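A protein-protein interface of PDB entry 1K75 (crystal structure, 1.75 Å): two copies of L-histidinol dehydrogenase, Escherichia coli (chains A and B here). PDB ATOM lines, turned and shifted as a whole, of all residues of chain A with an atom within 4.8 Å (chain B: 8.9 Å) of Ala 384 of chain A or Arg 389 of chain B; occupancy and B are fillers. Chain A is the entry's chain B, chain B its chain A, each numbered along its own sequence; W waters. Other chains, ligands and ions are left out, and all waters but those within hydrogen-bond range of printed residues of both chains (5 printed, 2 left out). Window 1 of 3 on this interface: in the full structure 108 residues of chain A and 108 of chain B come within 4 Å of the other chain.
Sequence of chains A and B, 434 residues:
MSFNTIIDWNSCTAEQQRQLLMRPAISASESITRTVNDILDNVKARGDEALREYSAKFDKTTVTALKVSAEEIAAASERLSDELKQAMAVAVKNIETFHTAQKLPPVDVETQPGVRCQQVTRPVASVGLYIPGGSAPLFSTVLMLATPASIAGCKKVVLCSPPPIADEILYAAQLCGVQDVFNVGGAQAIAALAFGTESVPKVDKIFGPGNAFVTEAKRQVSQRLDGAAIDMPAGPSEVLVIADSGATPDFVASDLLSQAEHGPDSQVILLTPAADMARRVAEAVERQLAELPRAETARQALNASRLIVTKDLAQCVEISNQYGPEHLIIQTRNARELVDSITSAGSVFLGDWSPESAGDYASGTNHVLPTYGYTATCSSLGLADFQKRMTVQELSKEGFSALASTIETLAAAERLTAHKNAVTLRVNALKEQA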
ATOM      1  N   GLN A 102       8.436 -30.353  14.992  1.00  0.00           N
ATOM      2  CA  GLN A 102       7.106 -30.372  15.605  1.00  0.00           C
ATOM      3  C   GLN A 102       6.221 -31.503  15.048  1.00  0.00           C
ATOM      4  O   GLN A 102       5.063 -31.662  15.461  1.00  0.00           O
ATOM      5  CB  GLN A 102       6.388 -29.028  15.389  1.00  0.00           C
ATOM      6  CG  GLN A 102       7.001 -27.888  16.147  1.00  0.00           C
ATOM      7  CD  GLN A 102       6.456 -26.541  15.716  1.00  0.00           C
ATOM      8  OE1 GLN A 102       5.316 -26.440  15.283  1.00  0.00           O
ATOM      9  NE2 GLN A 102       7.270 -25.502  15.833  1.00  0.00           N
ATOM     10  N   GLY A 346       2.874 -16.464  24.825  1.00  0.00           N
ATOM     11  CA  GLY A 346       2.964 -16.969  23.450  1.00  0.00           C
ATOM     12  C   GLY A 346       4.348 -17.516  23.125  1.00  0.00           C
ATOM     13  O   GLY A 346       4.483 -18.673  22.718  1.00  0.00           O
ATOM     14  N   SER A 379      -2.308 -21.167  20.778  1.00  0.00           N
ATOM     15  CA  SER A 379      -0.865 -21.401  20.733  1.00  0.00           C
ATOM     16  C   SER A 379      -0.210 -20.587  19.658  1.00  0.00           C
ATOM     17  O   SER A 379      -0.854 -20.137  18.706  1.00  0.00           O
ATOM     18  CB  SER A 379      -0.559 -22.856  20.365  1.00  0.00           C
ATOM     19  OG  SER A 379      -1.261 -23.809  21.148  1.00  0.00           O
ATOM     20  N   SER A 380       1.103 -20.471  19.793  1.00  0.00           N
ATOM     21  CA  SER A 380       1.932 -19.856  18.791  1.00  0.00           C
ATOM     22  C   SER A 380       1.563 -20.601  17.496  1.00  0.00           C
ATOM     23  O   SER A 380       1.190 -21.784  17.543  1.00  0.00           O
ATOM     24  CB  SER A 380       3.401 -20.178  19.087  1.00  0.00           C
ATOM     25  OG  SER A 380       4.184 -19.993  17.907  1.00  0.00           O
ATOM     26  N   LEU A 381       1.623 -19.923  16.361  1.00  0.00           N
ATOM     27  CA  LEU A 381       1.362 -20.592  15.086  1.00  0.00           C
ATOM     28  C   LEU A 381       2.500 -21.631  14.999  1.00  0.00           C
ATOM     29  O   LEU A 381       3.635 -21.351  15.423  1.00  0.00           O
ATOM     30  CB  LEU A 381       1.498 -19.609  13.908  1.00  0.00           C
ATOM     31  CG  LEU A 381       0.946 -20.203  12.605  1.00  0.00           C
ATOM     32  CD1 LEU A 381      -0.586 -20.154  12.662  1.00  0.00           C
ATOM     33  CD2 LEU A 381       1.493 -19.411  11.390  1.00  0.00           C
ATOM     34  N   GLY A 382       2.197 -22.817  14.487  1.00  0.00           N
ATOM     35  CA  GLY A 382       3.224 -23.852  14.342  1.00  0.00           C
ATOM     36  C   GLY A 382       2.759 -24.794  13.248  1.00  0.00           C
ATOM     37  O   GLY A 382       1.795 -24.482  12.560  1.00  0.00           O
ATOM     38  N   LEU A 383       3.429 -25.939  13.095  1.00  0.00           N
ATOM     39  CA  LEU A 383       3.077 -26.910  12.071  1.00  0.00           C
ATOM     40  C   LEU A 383       1.601 -27.335  12.215  1.00  0.00           C
ATOM     41  O   LEU A 383       0.865 -27.473  11.229  1.00  0.00           O
ATOM     42  CB  LEU A 383       3.978 -28.139  12.221  1.00  0.00           C
ATOM     43  CG  LEU A 383       3.767 -29.269  11.208  1.00  0.00           C
ATOM     44  CD1 LEU A 383       4.030 -28.770   9.781  1.00  0.00           C
ATOM     45  CD2 LEU A 383       4.763 -30.407  11.562  1.00  0.00           C
ATOM     46  N   ALA A 384       1.195 -27.529  13.460  1.00  0.00           N
ATOM     47  CA  ALA A 384      -0.162 -27.964  13.783  1.00  0.00           C
ATOM     48  C   ALA A 384      -1.265 -27.118  13.140  1.00  0.00           C
ATOM     49  O   ALA A 384      -2.342 -27.641  12.812  1.00  0.00           O
ATOM     50  CB  ALA A 384      -0.327 -27.983  15.290  1.00  0.00           C
ATOM     51  N   ASP A 385      -1.007 -25.824  12.945  1.00  0.00           N
ATOM     52  CA  ASP A 385      -2.023 -24.943  12.358  1.00  0.00           C
ATOM     53  C   ASP A 385      -2.249 -25.168  10.862  1.00  0.00           C
ATOM     54  O   ASP A 385      -3.202 -24.655  10.278  1.00  0.00           O
ATOM     55  CB  ASP A 385      -1.640 -23.504  12.600  1.00  0.00           C
ATOM     56  CG  ASP A 385      -1.580 -23.187  14.067  1.00  0.00           C
ATOM     57  OD1 ASP A 385      -2.663 -22.890  14.642  1.00  0.00           O
ATOM     58  OD2 ASP A 385      -0.474 -23.285  14.644  1.00  0.00           O
ATOM     59  N   PHE A 386      -1.371 -25.946  10.251  1.00  0.00           N
ATOM     60  CA  PHE A 386      -1.480 -26.244   8.819  1.00  0.00           C
ATOM     61  C   PHE A 386      -1.943 -27.698   8.589  1.00  0.00           C
ATOM     62  O   PHE A 386      -1.931 -28.183   7.454  1.00  0.00           O
ATOM     63  CB  PHE A 386      -0.126 -26.019   8.129  1.00  0.00           C
ATOM     64  CG  PHE A 386       0.312 -24.598   8.145  1.00  0.00           C
ATOM     65  CD1 PHE A 386       0.907 -24.052   9.295  1.00  0.00           C
ATOM     66  CD2 PHE A 386       0.068 -23.766   7.047  1.00  0.00           C
ATOM     67  CE1 PHE A 386       1.246 -22.666   9.335  1.00  0.00           C
ATOM     68  CE2 PHE A 386       0.410 -22.387   7.092  1.00  0.00           C
ATOM     69  CZ  PHE A 386       0.994 -21.851   8.240  1.00  0.00           C
ATOM     70  N   GLN A 387      -2.329 -28.369   9.664  1.00  0.00           N
ATOM     71  CA  GLN A 387      -2.797 -29.747   9.546  1.00  0.00           C
ATOM     72  C   GLN A 387      -3.979 -30.079  10.469  1.00  0.00           C
ATOM     73  O   GLN A 387      -4.473 -29.226  11.225  1.00  0.00           O
ATOM     74  CB  GLN A 387      -1.611 -30.721   9.742  1.00  0.00           C
ATOM     75  CG  GLN A 387      -0.843 -30.539  11.014  1.00  0.00           C
ATOM     76  CD  GLN A 387       0.472 -31.369  11.116  1.00  0.00           C
ATOM     77  OE1 GLN A 387       0.922 -31.622  12.213  1.00  0.00           O
ATOM     78  NE2 GLN A 387       1.059 -31.771   9.999  1.00  0.00           N
ATOM     79  N   LEU B 104       2.150 -34.657  23.367  1.00  0.00           N
ATOM     80  CA  LEU B 104       3.198 -34.203  22.442  1.00  0.00           C
ATOM     81  C   LEU B 104       4.554 -34.430  23.082  1.00  0.00           C
ATOM     82  O   LEU B 104       4.820 -33.916  24.168  1.00  0.00           O
ATOM     83  CB  LEU B 104       3.072 -32.707  22.137  1.00  0.00           C
ATOM     84  CG  LEU B 104       1.785 -32.169  21.523  1.00  0.00           C
ATOM     85  CD1 LEU B 104       1.938 -30.680  21.224  1.00  0.00           C
ATOM     86  CD2 LEU B 104       1.481 -32.950  20.245  1.00  0.00           C
ATOM     87  N   PRO B 105       5.429 -35.212  22.434  1.00  0.00           N
ATOM     88  CA  PRO B 105       6.735 -35.413  23.071  1.00  0.00           C
ATOM     89  C   PRO B 105       7.499 -34.074  23.095  1.00  0.00           C
ATOM     90  O   PRO B 105       7.143 -33.121  22.405  1.00  0.00           O
ATOM     91  CB  PRO B 105       7.412 -36.450  22.168  1.00  0.00           C
ATOM     92  CG  PRO B 105       6.281 -37.133  21.503  1.00  0.00           C
ATOM     93  CD  PRO B 105       5.325 -36.013  21.203  1.00  0.00           C
ATOM     94  N   VAL B 107       9.891 -31.003  22.384  1.00  0.00           N
ATOM     95  CA  VAL B 107      10.537 -30.465  21.191  1.00  0.00           C
ATOM     96  C   VAL B 107      11.635 -29.576  21.753  1.00  0.00           C
ATOM     97  O   VAL B 107      11.347 -28.602  22.431  1.00  0.00           O
ATOM     98  CB  VAL B 107       9.577 -29.620  20.338  1.00  0.00           C
ATOM     99  CG1 VAL B 107      10.343 -29.017  19.151  1.00  0.00           C
ATOM    100  CG2 VAL B 107       8.396 -30.494  19.878  1.00  0.00           C
ATOM    101  N   GLN B 118      12.539 -24.423  21.797  1.00  0.00           N
ATOM    102  CA  GLN B 118      11.696 -25.467  22.360  1.00  0.00           C
ATOM    103  C   GLN B 118      10.218 -25.193  22.178  1.00  0.00           C
ATOM    104  O   GLN B 118       9.790 -24.052  21.988  1.00  0.00           O
ATOM    105  CB  GLN B 118      11.923 -25.592  23.860  1.00  0.00           C
ATOM    106  CG  GLN B 118      13.291 -26.068  24.309  1.00  0.00           C
ATOM    107  CD  GLN B 118      13.465 -25.864  25.799  1.00  0.00           C
ATOM    108  OE1 GLN B 118      13.081 -26.707  26.637  1.00  0.00           O
ATOM    109  NE2 GLN B 118      13.999 -24.734  26.143  1.00  0.00           N
ATOM    110  N   GLN B 119       9.450 -26.267  22.257  1.00  0.00           N
ATOM    111  CA  GLN B 119       8.018 -26.176  22.211  1.00  0.00           C
ATOM    112  C   GLN B 119       7.552 -26.964  23.403  1.00  0.00           C
ATOM    113  O   GLN B 119       7.859 -28.158  23.549  1.00  0.00           O
ATOM    114  CB  GLN B 119       7.465 -26.783  20.937  1.00  0.00           C
ATOM    115  CG  GLN B 119       5.974 -26.670  20.846  1.00  0.00           C
ATOM    116  CD  GLN B 119       5.438 -27.514  19.713  1.00  0.00           C
ATOM    117  OE1 GLN B 119       5.273 -28.732  19.849  1.00  0.00           O
ATOM    118  NE2 GLN B 119       5.193 -26.888  18.586  1.00  0.00           N
ATOM    119  N   VAL B 120       6.872 -26.289  24.307  1.00  0.00           N
ATOM    120  CA  VAL B 120       6.371 -26.992  25.458  1.00  0.00           C
ATOM    121  C   VAL B 120       4.866 -26.837  25.489  1.00  0.00           C
ATOM    122  O   VAL B 120       4.289 -26.062  24.703  1.00  0.00           O
ATOM    123  CB  VAL B 120       6.973 -26.451  26.780  1.00  0.00           C
ATOM    124  CG1 VAL B 120       8.493 -26.695  26.805  1.00  0.00           C
ATOM    125  CG2 VAL B 120       6.683 -24.979  26.929  1.00  0.00           C
ATOM    126  N   THR B 121       4.226 -27.587  26.378  1.00  0.00           N
ATOM    127  CA  THR B 121       2.786 -27.487  26.477  1.00  0.00           C
ATOM    128  C   THR B 121       2.358 -27.034  27.872  1.00  0.00           C
ATOM    129  O   THR B 121       3.030 -27.272  28.882  1.00  0.00           O
ATOM    130  CB  THR B 121       2.104 -28.840  26.157  1.00  0.00           C
ATOM    131  OG1 THR B 121       2.587 -29.824  27.060  1.00  0.00           O
ATOM    132  CG2 THR B 121       2.425 -29.279  24.718  1.00  0.00           C
ATOM    133  N   ARG B 122       1.216 -26.364  27.899  1.00  0.00           N
ATOM    134  CA  ARG B 122       0.652 -25.892  29.140  1.00  0.00           C
ATOM    135  C   ARG B 122      -0.852 -26.142  29.016  1.00  0.00           C
ATOM    136  O   ARG B 122      -1.435 -25.953  27.952  1.00  0.00           O
ATOM    137  CB  ARG B 122       0.923 -24.395  29.313  1.00  0.00           C
ATOM    138  CG  ARG B 122       2.381 -24.060  29.594  1.00  0.00           C
ATOM    139  CD  ARG B 122       2.819 -24.625  30.917  1.00  0.00           C
ATOM    140  NE  ARG B 122       4.186 -24.243  31.273  1.00  0.00           N
ATOM    141  CZ  ARG B 122       5.275 -24.910  30.893  1.00  0.00           C
ATOM    142  NH1 ARG B 122       5.158 -26.002  30.131  1.00  0.00           N
ATOM    143  NH2 ARG B 122       6.484 -24.500  31.300  1.00  0.00           N
ATOM    144  N   PRO B 123      -1.492 -26.555  30.106  1.00  0.00           N
ATOM    145  CA  PRO B 123      -2.935 -26.803  30.028  1.00  0.00           C
ATOM    146  C   PRO B 123      -3.775 -25.534  29.975  1.00  0.00           C
ATOM    147  O   PRO B 123      -3.325 -24.451  30.390  1.00  0.00           O
ATOM    148  CB  PRO B 123      -3.208 -27.598  31.308  1.00  0.00           C
ATOM    149  CG  PRO B 123      -2.239 -26.972  32.285  1.00  0.00           C
ATOM    150  CD  PRO B 123      -0.967 -26.925  31.427  1.00  0.00           C
ATOM    151  N   VAL B 124      -4.993 -25.655  29.442  1.00  0.00           N
ATOM    152  CA  VAL B 124      -5.917 -24.528  29.464  1.00  0.00           C
ATOM    153  C   VAL B 124      -6.281 -24.565  30.955  1.00  0.00           C
ATOM    154  O   VAL B 124      -6.615 -25.616  31.502  1.00  0.00           O
ATOM    155  CB  VAL B 124      -7.132 -24.797  28.536  1.00  0.00           C
ATOM    156  CG1 VAL B 124      -8.231 -23.761  28.750  1.00  0.00           C
ATOM    157  CG2 VAL B 124      -6.663 -24.751  27.084  1.00  0.00           C
ATOM    158  N   THR B 377     -10.687 -28.086   8.140  1.00  0.00           N
ATOM    159  CA  THR B 377      -9.535 -27.606   8.905  1.00  0.00           C
ATOM    160  C   THR B 377      -9.523 -27.979  10.382  1.00  0.00           C
ATOM    161  O   THR B 377      -8.526 -27.758  11.067  1.00  0.00           O
ATOM    162  CB  THR B 377      -9.426 -26.072   8.818  1.00  0.00           C
ATOM    163  OG1 THR B 377     -10.500 -25.489   9.559  1.00  0.00           O
ATOM    164  CG2 THR B 377      -9.532 -25.593   7.353  1.00  0.00           C
ATOM    165  N   CYS B 378     -10.624 -28.526  10.886  1.00  0.00           N
ATOM    166  CA  CYS B 378     -10.698 -28.866  12.306  1.00  0.00           C
ATOM    167  C   CYS B 378     -10.435 -30.336  12.504  1.00  0.00           C
ATOM    168  O   CYS B 378     -10.632 -31.139  11.591  1.00  0.00           O
ATOM    169  CB  CYS B 378     -12.093 -28.550  12.874  1.00  0.00           C
ATOM    170  SG  CYS B 378     -12.517 -26.778  12.796  1.00  0.00           S
ATOM    171  N   SER B 379     -10.043 -30.666  13.718  1.00  0.00           N
ATOM    172  CA  SER B 379      -9.756 -32.036  14.107  1.00  0.00           C
ATOM    173  C   SER B 379     -10.739 -32.582  15.123  1.00  0.00           C
ATOM    174  O   SER B 379     -11.493 -31.848  15.766  1.00  0.00           O
ATOM    175  CB  SER B 379      -8.376 -32.089  14.748  1.00  0.00           C
ATOM    176  OG  SER B 379      -7.385 -31.709  13.790  1.00  0.00           O
ATOM    177  N   ALA B 384      -4.970 -32.226  22.675  1.00  0.00           N
ATOM    178  CA  ALA B 384      -4.530 -30.913  22.214  1.00  0.00           C
ATOM    179  C   ALA B 384      -5.538 -29.784  22.475  1.00  0.00           C
ATOM    180  O   ALA B 384      -5.138 -28.653  22.741  1.00  0.00           O
ATOM    181  CB  ALA B 384      -4.193 -30.976  20.721  1.00  0.00           C
ATOM    182  N   PHE B 386      -7.277 -29.251  24.977  1.00  0.00           N
ATOM    183  CA  PHE B 386      -7.299 -28.869  26.387  1.00  0.00           C
ATOM    184  C   PHE B 386      -5.961 -28.278  26.811  1.00  0.00           C
ATOM    185  O   PHE B 386      -5.692 -28.096  28.001  1.00  0.00           O
ATOM    186  CB  PHE B 386      -7.617 -30.083  27.232  1.00  0.00           C
ATOM    187  CG  PHE B 386      -9.008 -30.595  27.024  1.00  0.00           C
ATOM    188  CD1 PHE B 386      -9.307 -31.444  25.957  1.00  0.00           C
ATOM    189  CD2 PHE B 386     -10.032 -30.188  27.876  1.00  0.00           C
ATOM    190  CE1 PHE B 386     -10.631 -31.891  25.737  1.00  0.00           C
ATOM    191  CE2 PHE B 386     -11.355 -30.617  27.671  1.00  0.00           C
ATOM    192  CZ  PHE B 386     -11.644 -31.475  26.591  1.00  0.00           C
ATOM    193  N   GLN B 387      -5.133 -27.984  25.825  1.00  0.00           N
ATOM    194  CA  GLN B 387      -3.810 -27.418  26.108  1.00  0.00           C
ATOM    195  C   GLN B 387      -3.330 -26.437  25.043  1.00  0.00           C
ATOM    196  O   GLN B 387      -4.004 -26.196  24.047  1.00  0.00           O
ATOM    197  CB  GLN B 387      -2.797 -28.539  26.316  1.00  0.00           C
ATOM    198  CG  GLN B 387      -2.601 -29.414  25.127  1.00  0.00           C
ATOM    199  CD  GLN B 387      -1.784 -30.685  25.431  1.00  0.00           C
ATOM    200  OE1 GLN B 387      -1.297 -31.337  24.512  1.00  0.00           O
ATOM    201  NE2 GLN B 387      -1.664 -31.042  26.701  1.00  0.00           N
ATOM    202  N   LYS B 388      -2.166 -25.839  25.287  1.00  0.00           N
ATOM    203  CA  LYS B 388      -1.605 -24.850  24.365  1.00  0.00           C
ATOM    204  C   LYS B 388      -0.110 -25.125  24.198  1.00  0.00           C
ATOM    205  O   LYS B 388       0.514 -25.616  25.117  1.00  0.00           O
ATOM    206  CB  LYS B 388      -1.740 -23.452  24.954  1.00  0.00           C
ATOM    207  CG  LYS B 388      -3.120 -23.057  25.355  1.00  0.00           C
ATOM    208  CD  LYS B 388      -3.044 -21.839  26.282  1.00  0.00           C
ATOM    209  CE  LYS B 388      -2.396 -22.172  27.629  1.00  0.00           C
ATOM    210  NZ  LYS B 388      -2.105 -20.905  28.376  1.00  0.00           N
ATOM    211  N   ARG B 389       0.421 -24.806  23.016  1.00  0.00           N
ATOM    212  CA  ARG B 389       1.854 -24.973  22.716  1.00  0.00           C
ATOM    213  C   ARG B 389       2.509 -23.609  22.977  1.00  0.00           C
ATOM    214  O   ARG B 389       2.021 -22.593  22.520  1.00  0.00           O
ATOM    215  CB  ARG B 389       2.072 -25.368  21.251  1.00  0.00           C
ATOM    216  CG  ARG B 389       1.621 -26.791  20.870  1.00  0.00           C
ATOM    217  CD  ARG B 389       1.657 -27.049  19.363  1.00  0.00           C
ATOM    218  NE  ARG B 389       0.540 -26.416  18.657  1.00  0.00           N
ATOM    219  CZ  ARG B 389       0.666 -25.372  17.839  1.00  0.00           C
ATOM    220  NH1 ARG B 389       1.864 -24.842  17.622  1.00  0.00           N
ATOM    221  NH2 ARG B 389      -0.409 -24.852  17.233  1.00  0.00           N
ATOM    222  N   MET B 390       3.559 -23.601  23.774  1.00  0.00           N
ATOM    223  CA  MET B 390       4.283 -22.373  24.109  1.00  0.00           C
ATOM    224  C   MET B 390       5.705 -22.524  23.566  1.00  0.00           C
ATOM    225  O   MET B 390       6.320 -23.562  23.751  1.00  0.00           O
ATOM    226  CB  MET B 390       4.304 -22.210  25.620  1.00  0.00           C
ATOM    227  CG  MET B 390       5.041 -21.024  26.107  1.00  0.00           C
ATOM    228  SD  MET B 390       4.556 -20.546  27.912  1.00  0.00           S
ATOM    229  CE  MET B 390       5.743 -21.814  28.853  1.00  0.00           C
ATOM    230  N   THR B 391       6.213 -21.496  22.917  1.00  0.00           N
ATOM    231  CA  THR B 391       7.556 -21.531  22.339  1.00  0.00           C
ATOM    232  C   THR B 391       8.558 -20.894  23.313  1.00  0.00           C
ATOM    233  O   THR B 391       8.236 -19.937  24.028  1.00  0.00           O
ATOM    234  CB  THR B 391       7.513 -20.789  20.966  1.00  0.00           C
ATOM    235  OG1 THR B 391       6.874 -21.661  20.018  1.00  0.00           O
ATOM    236  CG2 THR B 391       8.862 -20.443  20.483  1.00  0.00           C
ATOM    237  N   VAL B 392       9.745 -21.472  23.398  1.00  0.00           N
ATOM    238  CA  VAL B 392      10.770 -20.923  24.289  1.00  0.00           C
ATOM    239  C   VAL B 392      12.104 -20.920  23.518  1.00  0.00           C
ATOM    240  O   VAL B 392      12.401 -21.870  22.783  1.00  0.00           O
ATOM    241  CB  VAL B 392      10.955 -21.793  25.566  1.00  0.00           C
ATOM    242  CG1 VAL B 392      12.052 -21.162  26.486  1.00  0.00           C
ATOM    243  CG2 VAL B 392       9.644 -21.955  26.303  1.00  0.00           C
HETATM  244  O   HOH W   1       2.373 -20.171  22.313  1.00  0.00           O
HETATM  245  O   HOH W   2      -3.925 -24.230  21.623  1.00  0.00           O
HETATM  246  O   HOH W   3       4.657 -30.990  18.045  1.00  0.00           O
HETATM  247  O   HOH W   4      -7.253 -29.032  13.085  1.00  0.00           O
HETATM  248  O   HOH W   5       6.824 -19.922  17.901  1.00  0.00           O
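The side-chain amide nitrogen (NE2) of Gln 119 of chain B lies close to the side-chain amide oxygen (OE1) of Gln 102 of chain A, 3.3 Å away.
NH2 of Arg 389 of chain B lies within salt-bridge range of OD2 of Asp 385 of chain A.
The backbone carbonyl oxygen (O) of Ser 380 of chain A is in hydrogen-bond range of the guanidinium group (NH1) of Arg 389 of chain B, 3.1 Å away.
The backbone NH (N) of Thr 391 of chain B is in hydrogen-bond range of the backbone carbonyl oxygen (O) of Gly 346 of chain A, 3.3 Å away.
N of Arg 389 of chain B lies within hydrogen-bond range of OG of Ser 379 of chain A (2.7 Å).
The backbone carbonyl oxygen (O) of Arg 122 of chain B lies within hydrogen-bond range of the backbone NH (N) of Lys 388 of chain B, at 2.8 Å.
The backbone NH (N) of Gly 382 of chain A lies within hydrogen-bond range of the side-chain carboxylate (OD2) of Asp 385 of chain A (2.7 Å).
O of Val 107 of chain B lies within hydrogen-bond range of N of Gln 119 of chain B (3.0 Å).
The backbone carbonyl oxygen of Val 120 of chain B is in hydrogen-bond range of the backbone NH of Met 390 of chain B (2.7 Å).
N of Leu 383 of chain A sits at hydrogen-bond distance from OE1 of Gln 102 of chain A (2.9 Å).
Among the printed residues, pairs that only touch across the chains: Gly 346 of chain A with Met 390 of chain B, Ser 379 of chain A with Lys 388 of chain B, Ser 380 of chain A with Thr 391 of chain B, Gly 382 of chain A with Arg 389 of chain B and Ala 384 of chain A with Arg 389 of chain B.
Of the printed residues of chain B, Ser 379 of chain A touches Lys 388 (3.4 Å) and Arg 389 (2.7 Å).
Printed residues of chain B within 4 Å of Ser 380 of chain A: Arg 389 (3.1 Å) and Thr 391 (3.8 Å).
Ala 384 of chain A touches just one residue of chain B: Arg 389.
Asp 385 of chain A touches just one residue of chain B: Arg 389 (3.0 Å).
Printed residues of chain A within 4 Å of Lys 388 of chain B: Ser 379.
Of chain A, only Ser 379 (2.7 Å), Ser 380 (3.1 Å), Gly 382 (3.7 Å), Ala 384 (3.7 Å) and Asp 385 (3.0 Å) come within 4 Å of Arg 389 of chain B.
Printed residues of chain A within 4 Å of Thr 391 of chain B: Gly 346 and Ser 380.
The nearest printed residue of chain A that does not touch Lys 388 of chain B is Ser 380 of chain A (6.5 Å).
Of the 11 printed residues of chain A, 7 touch a printed residue of chain B.
Hydrophobic or aromatic side chains of chain A within 4 Å of the printed part of chain B: Ala 384.
Of the 21 printed residues of chain B, 5 touch a printed residue of chain A.
Printed residues of chain B that touch a printed residue of chain A: Gln 119, Lys 388, Arg 389, Met 390 and Thr 391.
Positions printed for both chains: 379, 384, 386 and 387.
Of the 10 pairs that touch across the chains among the printed residues, none has its exchanged pair printed and touching as well.
Water W1 lies within hydrogen-bond range of the backbone carbonyl oxygen of Arg 389 of chain B, the backbone carbonyl oxygen of Gly 346 of chain A and the backbone NH of Ser 380 of chain A.
Water W5 lies within hydrogen-bond range of OG of Ser 380 of chain A (2.6 Å) and OG1 of Thr 391 of chain B (2.7 Å).
Water W3 lies within hydrogen-bond range of O of Gln 102 of chain A (2.7 Å) and OE1 of Gln 119 of chain B (3.0 Å).
Water W4 lies within hydrogen-bond range of the backbone carbonyl oxygen of Thr 377 of chain B (2.7 Å), the side-chain hydroxyl of Ser 379 of chain B (2.8 Å) and the backbone carbonyl oxygen of Gln 387 of chain A (3.4 Å).
Water W2 bridges the side-chain hydroxyl (OG) of Ser 379 of chain A (2.7 Å) and the backbone carbonyl oxygen (O) of Gln 387 of chain B (3.1 Å).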
